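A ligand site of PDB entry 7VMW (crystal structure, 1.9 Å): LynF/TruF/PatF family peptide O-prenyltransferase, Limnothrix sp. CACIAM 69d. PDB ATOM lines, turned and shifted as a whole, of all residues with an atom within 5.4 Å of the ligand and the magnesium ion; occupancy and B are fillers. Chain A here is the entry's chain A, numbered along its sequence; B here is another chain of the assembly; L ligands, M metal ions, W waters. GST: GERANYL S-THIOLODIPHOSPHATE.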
ATOM      1  N   GLU A  54       7.458 -23.961  22.521  1.00  0.00           N
ATOM      2  CA  GLU A  54       6.463 -23.424  21.594  1.00  0.00           C
ATOM      3  C   GLU A  54       5.179 -24.219  21.785  1.00  0.00           C
ATOM      4  O   GLU A  54       5.199 -25.441  21.610  1.00  0.00           O
ATOM      5  CB  GLU A  54       6.983 -23.528  20.155  1.00  0.00           C
ATOM      6  CG  GLU A  54       5.989 -23.099  19.081  1.00  0.00           C
ATOM      7  CD  GLU A  54       6.312 -23.689  17.712  1.00  0.00           C
ATOM      8  OE1 GLU A  54       6.084 -24.936  17.479  1.00  0.00           O
ATOM      9  OE2 GLU A  54       6.860 -22.886  16.896  1.00  0.00           O
ATOM     10  N   LYS A  58      -4.093 -26.176  16.462  1.00  0.00           N
ATOM     11  CA  LYS A  58      -4.635 -26.413  15.131  1.00  0.00           C
ATOM     12  C   LYS A  58      -6.158 -26.306  15.169  1.00  0.00           C
ATOM     13  O   LYS A  58      -6.803 -27.006  15.964  1.00  0.00           O
ATOM     14  CB  LYS A  58      -4.210 -27.795  14.612  1.00  0.00           C
ATOM     15  CG  LYS A  58      -4.878 -28.155  13.270  1.00  0.00           C
ATOM     16  CD  LYS A  58      -4.583 -29.600  12.940  1.00  0.00           C
ATOM     17  CE  LYS A  58      -3.145 -29.751  12.516  1.00  0.00           C
ATOM     18  NZ  LYS A  58      -2.775 -28.788  11.459  1.00  0.00           N
ATOM     19  N   ARG A  68      -0.205 -29.770  21.183  1.00  0.00           N
ATOM     20  CA  ARG A  68       0.895 -29.518  20.252  1.00  0.00           C
ATOM     21  C   ARG A  68       1.952 -28.669  20.949  1.00  0.00           C
ATOM     22  O   ARG A  68       1.708 -27.494  21.268  1.00  0.00           O
ATOM     23  CB  ARG A  68       0.418 -28.841  18.958  1.00  0.00           C
ATOM     24  CG  ARG A  68      -0.629 -29.666  18.158  1.00  0.00           C
ATOM     25  CD  ARG A  68      -1.392 -28.861  17.060  1.00  0.00           C
ATOM     26  NE  ARG A  68      -0.510 -27.984  16.292  1.00  0.00           N
ATOM     27  CZ  ARG A  68       0.034 -28.335  15.133  1.00  0.00           C
ATOM     28  NH1 ARG A  68      -0.244 -29.498  14.572  1.00  0.00           N
ATOM     29  NH2 ARG A  68       0.893 -27.507  14.540  1.00  0.00           N
ATOM     30  N   ASP A  70       6.339 -28.004  20.903  1.00  0.00           N
ATOM     31  CA  ASP A  70       7.689 -28.258  20.410  1.00  0.00           C
ATOM     32  C   ASP A  70       8.717 -27.668  21.376  1.00  0.00           C
ATOM     33  O   ASP A  70       8.518 -26.566  21.930  1.00  0.00           O
ATOM     34  CB  ASP A  70       7.925 -27.643  19.027  1.00  0.00           C
ATOM     35  CG  ASP A  70       7.079 -28.275  17.905  1.00  0.00           C
ATOM     36  OD1 ASP A  70       6.804 -29.499  17.904  1.00  0.00           O
ATOM     37  OD2 ASP A  70       6.751 -27.555  16.935  1.00  0.00           O
ATOM     38  N   ASP A 126       2.164 -33.934  18.700  1.00  0.00           N
ATOM     39  CA  ASP A 126       0.783 -33.481  18.377  1.00  0.00           C
ATOM     40  C   ASP A 126      -0.184 -34.637  18.685  1.00  0.00           C
ATOM     41  O   ASP A 126      -0.370 -35.528  17.852  1.00  0.00           O
ATOM     42  CB  ASP A 126       0.623 -33.060  16.918  1.00  0.00           C
ATOM     43  CG  ASP A 126      -0.810 -32.618  16.585  1.00  0.00           C
ATOM     44  OD1 ASP A 126      -1.800 -32.827  17.380  1.00  0.00           O
ATOM     45  OD2 ASP A 126      -0.988 -32.019  15.489  1.00  0.00           O
ATOM     46  N   LYS A 135       0.912 -38.115  16.833  1.00  0.00           N
ATOM     47  CA  LYS A 135       2.260 -38.240  16.259  1.00  0.00           C
ATOM     48  C   LYS A 135       3.316 -37.558  17.125  1.00  0.00           C
ATOM     49  O   LYS A 135       3.015 -36.673  17.925  1.00  0.00           O
ATOM     50  CB  LYS A 135       2.298 -37.654  14.835  1.00  0.00           C
ATOM     51  CG  LYS A 135       2.002 -36.142  14.766  1.00  0.00           C
ATOM     52  CD  LYS A 135       1.796 -35.673  13.247  1.00  0.00           C
ATOM     53  CE  LYS A 135       1.574 -34.184  13.099  1.00  0.00           C
ATOM     54  NZ  LYS A 135       1.232 -33.785  11.662  1.00  0.00           N
ATOM     55  N   LYS A 137       7.362 -35.767  16.778  1.00  0.00           N
ATOM     56  CA  LYS A 137       8.016 -34.895  15.813  1.00  0.00           C
ATOM     57  C   LYS A 137       9.490 -34.709  16.144  1.00  0.00           C
ATOM     58  O   LYS A 137       9.869 -34.621  17.329  1.00  0.00           O
ATOM     59  CB  LYS A 137       7.321 -33.533  15.767  1.00  0.00           C
ATOM     60  CG  LYS A 137       5.896 -33.578  15.246  1.00  0.00           C
ATOM     61  CD  LYS A 137       5.296 -32.165  15.285  1.00  0.00           C
ATOM     62  CE  LYS A 137       4.079 -32.042  14.370  1.00  0.00           C
ATOM     63  NZ  LYS A 137       4.416 -32.023  12.863  1.00  0.00           N
ATOM     64  N   PHE A 139      12.747 -32.185  14.398  1.00  0.00           N
ATOM     65  CA  PHE A 139      13.153 -31.239  13.369  1.00  0.00           C
ATOM     66  C   PHE A 139      14.657 -31.099  13.413  1.00  0.00           C
ATOM     67  O   PHE A 139      15.258 -31.069  14.502  1.00  0.00           O
ATOM     68  CB  PHE A 139      12.542 -29.840  13.546  1.00  0.00           C
ATOM     69  CG  PHE A 139      11.065 -29.794  13.471  1.00  0.00           C
ATOM     70  CD1 PHE A 139      10.306 -30.180  14.584  1.00  0.00           C
ATOM     71  CD2 PHE A 139      10.414 -29.288  12.337  1.00  0.00           C
ATOM     72  CE1 PHE A 139       8.911 -30.103  14.570  1.00  0.00           C
ATOM     73  CE2 PHE A 139       9.017 -29.209  12.313  1.00  0.00           C
ATOM     74  CZ  PHE A 139       8.261 -29.598  13.436  1.00  0.00           C
ATOM     75  N   ARG A 141      17.627 -28.667  11.312  1.00  0.00           N
ATOM     76  CA  ARG A 141      18.035 -27.726  10.270  1.00  0.00           C
ATOM     77  C   ARG A 141      19.503 -27.951   9.947  1.00  0.00           C
ATOM     78  O   ARG A 141      20.327 -28.078  10.859  1.00  0.00           O
ATOM     79  CB  ARG A 141      17.780 -26.288  10.727  1.00  0.00           C
ATOM     80  CG  ARG A 141      18.190 -25.229   9.695  1.00  0.00           C
ATOM     81  CD  ARG A 141      18.102 -23.796  10.267  1.00  0.00           C
ATOM     82  NE  ARG A 141      16.714 -23.375  10.451  1.00  0.00           N
ATOM     83  CZ  ARG A 141      16.071 -22.593   9.592  1.00  0.00           C
ATOM     84  NH1 ARG A 141      16.667 -22.144   8.496  1.00  0.00           N
ATOM     85  NH2 ARG A 141      14.813 -22.241   9.851  1.00  0.00           N
ATOM     86  N   HIS A 172      15.479 -26.080   6.818  1.00  0.00           N
ATOM     87  CA  HIS A 172      14.731 -26.685   7.923  1.00  0.00           C
ATOM     88  C   HIS A 172      13.953 -27.929   7.462  1.00  0.00           C
ATOM     89  O   HIS A 172      13.216 -27.888   6.461  1.00  0.00           O
ATOM     90  CB  HIS A 172      13.770 -25.615   8.468  1.00  0.00           C
ATOM     91  CG  HIS A 172      13.245 -25.874   9.843  1.00  0.00           C
ATOM     92  ND1 HIS A 172      14.059 -26.031  10.931  1.00  0.00           N
ATOM     93  CD2 HIS A 172      11.964 -25.945  10.304  1.00  0.00           C
ATOM     94  CE1 HIS A 172      13.313 -26.204  12.014  1.00  0.00           C
ATOM     95  NE2 HIS A 172      12.040 -26.162  11.658  1.00  0.00           N
ATOM     96  N   ASP A 176       7.709 -36.505  10.860  1.00  0.00           N
ATOM     97  CA  ASP A 176       6.501 -36.843  11.625  1.00  0.00           C
ATOM     98  C   ASP A 176       6.437 -38.359  11.788  1.00  0.00           C
ATOM     99  O   ASP A 176       6.589 -39.067  10.776  1.00  0.00           O
ATOM    100  CB  ASP A 176       5.224 -36.410  10.873  1.00  0.00           C
ATOM    101  CG  ASP A 176       4.786 -34.966  11.166  1.00  0.00           C
ATOM    102  OD1 ASP A 176       5.452 -34.285  11.965  1.00  0.00           O
ATOM    103  OD2 ASP A 176       3.758 -34.511  10.568  1.00  0.00           O
ATOM    104  N   GLU A 186       8.913 -33.355   5.894  1.00  0.00           N
ATOM    105  CA  GLU A 186       8.503 -32.059   5.326  1.00  0.00           C
ATOM    106  C   GLU A 186       9.729 -31.154   5.202  1.00  0.00           C
ATOM    107  O   GLU A 186      10.539 -31.093   6.136  1.00  0.00           O
ATOM    108  CB  GLU A 186       7.415 -31.391   6.181  1.00  0.00           C
ATOM    109  CG  GLU A 186       6.848 -30.036   5.672  1.00  0.00           C
ATOM    110  CD  GLU A 186       5.446 -29.750   6.283  1.00  0.00           C
ATOM    111  OE1 GLU A 186       5.146 -30.290   7.372  1.00  0.00           O
ATOM    112  OE2 GLU A 186       4.649 -28.993   5.694  1.00  0.00           O
ATOM    113  N   TYR A 188      10.937 -27.130   4.642  1.00  0.00           N
ATOM    114  CA  TYR A 188      10.399 -25.776   4.819  1.00  0.00           C
ATOM    115  C   TYR A 188      11.333 -24.720   4.214  1.00  0.00           C
ATOM    116  O   TYR A 188      11.974 -23.968   4.953  1.00  0.00           O
ATOM    117  CB  TYR A 188      10.179 -25.482   6.305  1.00  0.00           C
ATOM    118  CG  TYR A 188       9.322 -26.480   7.076  1.00  0.00           C
ATOM    119  CD1 TYR A 188       9.906 -27.563   7.708  1.00  0.00           C
ATOM    120  CD2 TYR A 188       7.934 -26.315   7.180  1.00  0.00           C
ATOM    121  CE1 TYR A 188       9.153 -28.467   8.445  1.00  0.00           C
ATOM    122  CE2 TYR A 188       7.131 -27.208   7.944  1.00  0.00           C
ATOM    123  CZ  TYR A 188       7.772 -28.267   8.589  1.00  0.00           C
ATOM    124  OH  TYR A 188       7.058 -29.202   9.307  1.00  0.00           O
ATOM    125  N   PRO A 189      11.444 -24.641   2.880  1.00  0.00           N
ATOM    126  CA  PRO A 189      12.228 -23.541   2.295  1.00  0.00           C
ATOM    127  C   PRO A 189      11.655 -22.183   2.707  1.00  0.00           C
ATOM    128  O   PRO A 189      10.434 -22.031   2.881  1.00  0.00           O
ATOM    129  CB  PRO A 189      12.123 -23.760   0.788  1.00  0.00           C
ATOM    130  CG  PRO A 189      10.882 -24.601   0.591  1.00  0.00           C
ATOM    131  CD  PRO A 189      10.820 -25.495   1.853  1.00  0.00           C
ATOM    132  N   GLU A 190      12.555 -21.206   2.860  1.00  0.00           N
ATOM    133  CA  GLU A 190      12.232 -19.934   3.515  1.00  0.00           C
ATOM    134  C   GLU A 190      12.989 -18.779   2.877  1.00  0.00           C
ATOM    135  O   GLU A 190      13.987 -18.948   2.159  1.00  0.00           O
ATOM    136  CB  GLU A 190      12.585 -19.965   4.985  1.00  0.00           C
ATOM    137  CG  GLU A 190      14.094 -19.723   5.194  1.00  0.00           C
ATOM    138  CD  GLU A 190      14.598 -20.131   6.575  1.00  0.00           C
ATOM    139  OE1 GLU A 190      14.019 -21.083   7.156  1.00  0.00           O
ATOM    140  OE2 GLU A 190      15.600 -19.526   7.060  1.00  0.00           O
ATOM    141  N   LEU A 222      10.191 -13.387   8.437  1.00  0.00           N
ATOM    142  CA  LEU A 222      10.502 -14.674   7.804  1.00  0.00           C
ATOM    143  C   LEU A 222       9.243 -15.229   7.155  1.00  0.00           C
ATOM    144  O   LEU A 222       8.163 -15.161   7.749  1.00  0.00           O
ATOM    145  CB  LEU A 222      11.034 -15.695   8.830  1.00  0.00           C
ATOM    146  CG  LEU A 222      11.795 -16.918   8.307  1.00  0.00           C
ATOM    147  CD1 LEU A 222      12.977 -16.446   7.479  1.00  0.00           C
ATOM    148  CD2 LEU A 222      12.284 -17.799   9.468  1.00  0.00           C
ATOM    149  N   PHE A 223       9.386 -15.834   5.969  1.00  0.00           N
ATOM    150  CA  PHE A 223       8.271 -16.449   5.244  1.00  0.00           C
ATOM    151  C   PHE A 223       8.730 -17.780   4.676  1.00  0.00           C
ATOM    152  O   PHE A 223       9.875 -17.897   4.201  1.00  0.00           O
ATOM    153  CB  PHE A 223       7.785 -15.532   4.091  1.00  0.00           C
ATOM    154  CG  PHE A 223       6.772 -16.180   3.170  1.00  0.00           C
ATOM    155  CD1 PHE A 223       5.472 -16.403   3.595  1.00  0.00           C
ATOM    156  CD2 PHE A 223       7.104 -16.474   1.858  1.00  0.00           C
ATOM    157  CE1 PHE A 223       4.508 -16.978   2.765  1.00  0.00           C
ATOM    158  CE2 PHE A 223       6.166 -17.080   0.992  1.00  0.00           C
ATOM    159  CZ  PHE A 223       4.858 -17.327   1.434  1.00  0.00           C
ATOM    160  N   GLY A 224       7.865 -18.795   4.750  1.00  0.00           N
ATOM    161  CA  GLY A 224       8.242 -20.068   4.166  1.00  0.00           C
ATOM    162  C   GLY A 224       7.068 -20.894   3.699  1.00  0.00           C
ATOM    163  O   GLY A 224       5.898 -20.513   3.857  1.00  0.00           O
ATOM    164  N   ILE A 225       7.385 -22.015   3.055  1.00  0.00           N
ATOM    165  CA  ILE A 225       6.363 -22.900   2.489  1.00  0.00           C
ATOM    166  C   ILE A 225       6.695 -24.333   2.880  1.00  0.00           C
ATOM    167  O   ILE A 225       7.840 -24.772   2.713  1.00  0.00           O
ATOM    168  CB  ILE A 225       6.277 -22.738   0.962  1.00  0.00           C
ATOM    169  CG1 ILE A 225       5.783 -21.338   0.617  1.00  0.00           C
ATOM    170  CG2 ILE A 225       5.355 -23.785   0.336  1.00  0.00           C
ATOM    171  CD1 ILE A 225       5.710 -21.132  -0.881  1.00  0.00           C
ATOM    172  N   ASN A 231       0.962 -33.516   2.800  1.00  0.00           N
ATOM    173  CA  ASN A 231       0.120 -32.327   2.715  1.00  0.00           C
ATOM    174  C   ASN A 231      -0.859 -32.463   1.538  1.00  0.00           C
ATOM    175  O   ASN A 231      -0.497 -32.945   0.455  1.00  0.00           O
ATOM    176  CB  ASN A 231       0.973 -31.061   2.488  1.00  0.00           C
ATOM    177  CG  ASN A 231       1.850 -30.690   3.670  1.00  0.00           C
ATOM    178  OD1 ASN A 231       1.639 -31.157   4.787  1.00  0.00           O
ATOM    179  ND2 ASN A 231       2.863 -29.861   3.422  1.00  0.00           N
ATOM    180  N   TYR A 237       3.796 -20.338   5.576  1.00  0.00           N
ATOM    181  CA  TYR A 237       4.219 -20.010   6.943  1.00  0.00           C
ATOM    182  C   TYR A 237       4.639 -18.541   7.035  1.00  0.00           C
ATOM    183  O   TYR A 237       5.538 -18.127   6.298  1.00  0.00           O
ATOM    184  CB  TYR A 237       5.385 -20.867   7.406  1.00  0.00           C
ATOM    185  CG  TYR A 237       4.943 -22.298   7.747  1.00  0.00           C
ATOM    186  CD1 TYR A 237       4.879 -23.289   6.758  1.00  0.00           C
ATOM    187  CD2 TYR A 237       4.636 -22.647   9.039  1.00  0.00           C
ATOM    188  CE1 TYR A 237       4.468 -24.602   7.058  1.00  0.00           C
ATOM    189  CE2 TYR A 237       4.215 -23.956   9.375  1.00  0.00           C
ATOM    190  CZ  TYR A 237       4.119 -24.917   8.360  1.00  0.00           C
ATOM    191  OH  TYR A 237       3.714 -26.197   8.677  1.00  0.00           O
ATOM    192  N   TRP A 273       3.883 -17.511  14.927  1.00  0.00           N
ATOM    193  CA  TRP A 273       3.791 -18.082  13.589  1.00  0.00           C
ATOM    194  C   TRP A 273       2.312 -18.293  13.284  1.00  0.00           C
ATOM    195  O   TRP A 273       1.531 -18.644  14.167  1.00  0.00           O
ATOM    196  CB  TRP A 273       4.522 -19.442  13.444  1.00  0.00           C
ATOM    197  CG  TRP A 273       6.012 -19.457  13.374  1.00  0.00           C
ATOM    198  CD1 TRP A 273       6.876 -19.670  14.402  1.00  0.00           C
ATOM    199  CD2 TRP A 273       6.825 -19.337  12.185  1.00  0.00           C
ATOM    200  NE1 TRP A 273       8.180 -19.660  13.940  1.00  0.00           N
ATOM    201  CE2 TRP A 273       8.173 -19.480  12.590  1.00  0.00           C
ATOM    202  CE3 TRP A 273       6.542 -19.166  10.820  1.00  0.00           C
ATOM    203  CZ2 TRP A 273       9.235 -19.415  11.683  1.00  0.00           C
ATOM    204  CZ3 TRP A 273       7.595 -19.085   9.920  1.00  0.00           C
ATOM    205  CH2 TRP A 273       8.926 -19.213  10.354  1.00  0.00           C
ATOM    206  N   ASN A 290      -3.199 -23.049  11.732  1.00  0.00           N
ATOM    207  CA  ASN A 290      -2.390 -23.340  12.904  1.00  0.00           C
ATOM    208  C   ASN A 290      -1.809 -22.038  13.465  1.00  0.00           C
ATOM    209  O   ASN A 290      -1.278 -21.240  12.694  1.00  0.00           O
ATOM    210  CB  ASN A 290      -1.201 -24.247  12.556  1.00  0.00           C
ATOM    211  CG  ASN A 290      -1.614 -25.644  12.063  1.00  0.00           C
ATOM    212  OD1 ASN A 290      -2.741 -26.088  12.254  1.00  0.00           O
ATOM    213  ND2 ASN A 290      -0.666 -26.331  11.422  1.00  0.00           N
ATOM    214  N   TYR A 292       1.027 -20.492  16.518  1.00  0.00           N
ATOM    215  CA  TYR A 292       2.172 -20.903  17.364  1.00  0.00           C
ATOM    216  C   TYR A 292       2.714 -19.727  18.179  1.00  0.00           C
ATOM    217  O   TYR A 292       2.962 -18.640  17.627  1.00  0.00           O
ATOM    218  CB  TYR A 292       3.351 -21.504  16.524  1.00  0.00           C
ATOM    219  CG  TYR A 292       2.932 -22.516  15.474  1.00  0.00           C
ATOM    220  CD1 TYR A 292       2.315 -22.096  14.298  1.00  0.00           C
ATOM    221  CD2 TYR A 292       3.175 -23.861  15.624  1.00  0.00           C
ATOM    222  CE1 TYR A 292       1.954 -22.996  13.316  1.00  0.00           C
ATOM    223  CE2 TYR A 292       2.817 -24.764  14.651  1.00  0.00           C
ATOM    224  CZ  TYR A 292       2.191 -24.324  13.504  1.00  0.00           C
ATOM    225  OH  TYR A 292       1.827 -25.203  12.497  1.00  0.00           O
ATOM    226  N   HIS B   4      12.081 -22.341  15.536  1.00  0.00           N
ATOM    227  CA  HIS B   4      12.263 -22.771  14.152  1.00  0.00           C
ATOM    228  C   HIS B   4      13.094 -21.806  13.282  1.00  0.00           C
ATOM    229  O   HIS B   4      13.281 -22.095  12.063  1.00  0.00           O
ATOM    230  CB  HIS B   4      10.923 -23.000  13.430  1.00  0.00           C
ATOM    231  CG  HIS B   4      10.039 -24.039  14.059  1.00  0.00           C
ATOM    232  ND1 HIS B   4      10.195 -25.388  13.813  1.00  0.00           N
ATOM    233  CD2 HIS B   4       8.948 -23.915  14.853  1.00  0.00           C
ATOM    234  CE1 HIS B   4       9.246 -26.055  14.452  1.00  0.00           C
ATOM    235  NE2 HIS B   4       8.482 -25.184  15.094  1.00  0.00           N
HETATM  236  PA  GST L   1       1.463 -29.945  11.183  1.00  0.00           P
HETATM  237  O1A GST L   1       1.571 -31.082  12.174  1.00  0.00           O
HETATM  238  O2A GST L   1       0.131 -29.240  11.162  1.00  0.00           O
HETATM  239  O3A GST L   1       1.780 -30.412   9.775  1.00  0.00           O
HETATM  240  O1B GST L   1       2.454 -28.768  11.644  1.00  0.00           O
HETATM  241  PB  GST L   1       4.011 -28.670  11.299  1.00  0.00           P
HETATM  242  O2B GST L   1       4.380 -29.026   9.896  1.00  0.00           O
HETATM  243  O3B GST L   1       4.895 -29.268  12.378  1.00  0.00           O
HETATM  244  S1  GST L   1       4.406 -26.693  11.536  1.00  0.00           S
HETATM  245  C1  GST L   1       6.019 -26.662  12.420  1.00  0.00           C
HETATM  246  C2  GST L   1       6.815 -25.430  11.910  1.00  0.00           C
HETATM  247  C3  GST L   1       6.924 -24.095  11.953  1.00  0.00           C
HETATM  248  C10 GST L   1       5.970 -23.215  12.819  1.00  0.00           C
HETATM  249  C4  GST L   1       7.926 -23.136  11.229  1.00  0.00           C
HETATM  250  C5  GST L   1       8.838 -23.744  10.148  1.00  0.00           C
HETATM  251  C6  GST L   1       8.715 -22.898   8.848  1.00  0.00           C
HETATM  252  C7  GST L   1       9.773 -22.383   8.192  1.00  0.00           C
HETATM  253  C9  GST L   1      11.241 -22.567   8.618  1.00  0.00           C
HETATM  254  C8  GST L   1       9.520 -21.547   6.924  1.00  0.00           C
HETATM  255 MG    MG M   1       3.462 -30.342   8.608  1.00  0.00          MG
HETATM  256  O   HOH W   1       2.622 -31.739   7.181  1.00  0.00           O
HETATM  257  O   HOH W   2       0.287 -32.249   8.531  1.00  0.00           O
HETATM  258  O   HOH W   3       4.317 -31.954   9.645  1.00  0.00           O
HETATM  259  O   HOH W   4       2.782 -28.690   7.471  1.00  0.00           O
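CZ of Phe 139 touches O3B of the ligand (3.5 Å). Arg 141 touches the ligand. His 172 touches the ligand. Glu 190 touches the ligand. Gly 224 touches the ligand. Trp 273 touches the ligand (CG to C10, 3.8 Å). His 4 of chain B touches the ligand. Along chain A the residues within 4 Å of the ligand span positions 58 to 292.
Water W3 lies within hydrogen-bond range of OD2 of Asp 176 (2.8 Å) and NZ of Lys 137 (3.2 Å). Water W4 bridges OE2 of Glu 186 (2.6 Å) and OH of Tyr 237 (2.9 Å).
OH of Tyr 188 sits close to O2B of the ligand (2.7 Å). NZ of Lys 135 lies within salt-bridge range of O1A of the ligand. The side-chain amino group of Lys 137 is in salt-bridge range of an oxygen (O3B) of the ligand, 2.8 Å away. NZ of Lys 58 lies within salt-bridge range of O2A of the ligand (3.0 Å). OH of Tyr 237 sits close to S1 of the ligand (3.0 Å). O2A of the ligand is in hydrogen-bond range of ND2 of Asn 290, at 3.0 Å. OH of Tyr 292 lies close to S1 of the ligand (3.1 Å). The guanidinium group (NH1) of Arg 68 is in salt-bridge range of an oxygen (O1A) of the ligand (3.4 Å).
Merely in contact with the magnesium ion: Tyr 188. Within 4 Å of the magnesium ion: Glu 186 and Tyr 188.
The magnesium ion is bound by O3A of the ligand. O2B of the ligand binds the magnesium ion (2.1 Å). The magnesium ion is bound by the side-chain carboxylate (OE1) of Glu 186 (2.1 Å). Water W3 binds the magnesium ion (2.1 Å). Water W4 binds the magnesium ion (2.1 Å). Water W1 is bound to the magnesium ion (2.2 Å). The magnesium ion has six donor atoms within binding distance.
The side-chain carboxylate of Glu 186 lies close to the side-chain hydroxyl of Tyr 188, 2.9 Å away. N of Asp 126 is in hydrogen-bond range of O of Lys 135 (3.0 Å). OD1 of Asp 176 lies within salt-bridge range of NZ of Lys 137, 2.6 Å away. The side-chain amide oxygen (OD1) of Asn 290 is in hydrogen-bond range of the side-chain amino group (NZ) of Lys 58 (2.8 Å). O of Trp 273 sits at hydrogen-bond distance from N of Tyr 292. O of His 4 of chain B lies within hydrogen-bond range of NH2 of Arg 141 (2.7 Å). A ring nitrogen (NE2) of His 4 of chain B sits close to the side-chain carboxylate (OE2) of Glu 54 (3.3 Å). The side-chain carboxylate (OD2) of Asp 70 is in hydrogen-bond range of a ring nitrogen (NE2) of His 4 of chain B, 3.5 Å away.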
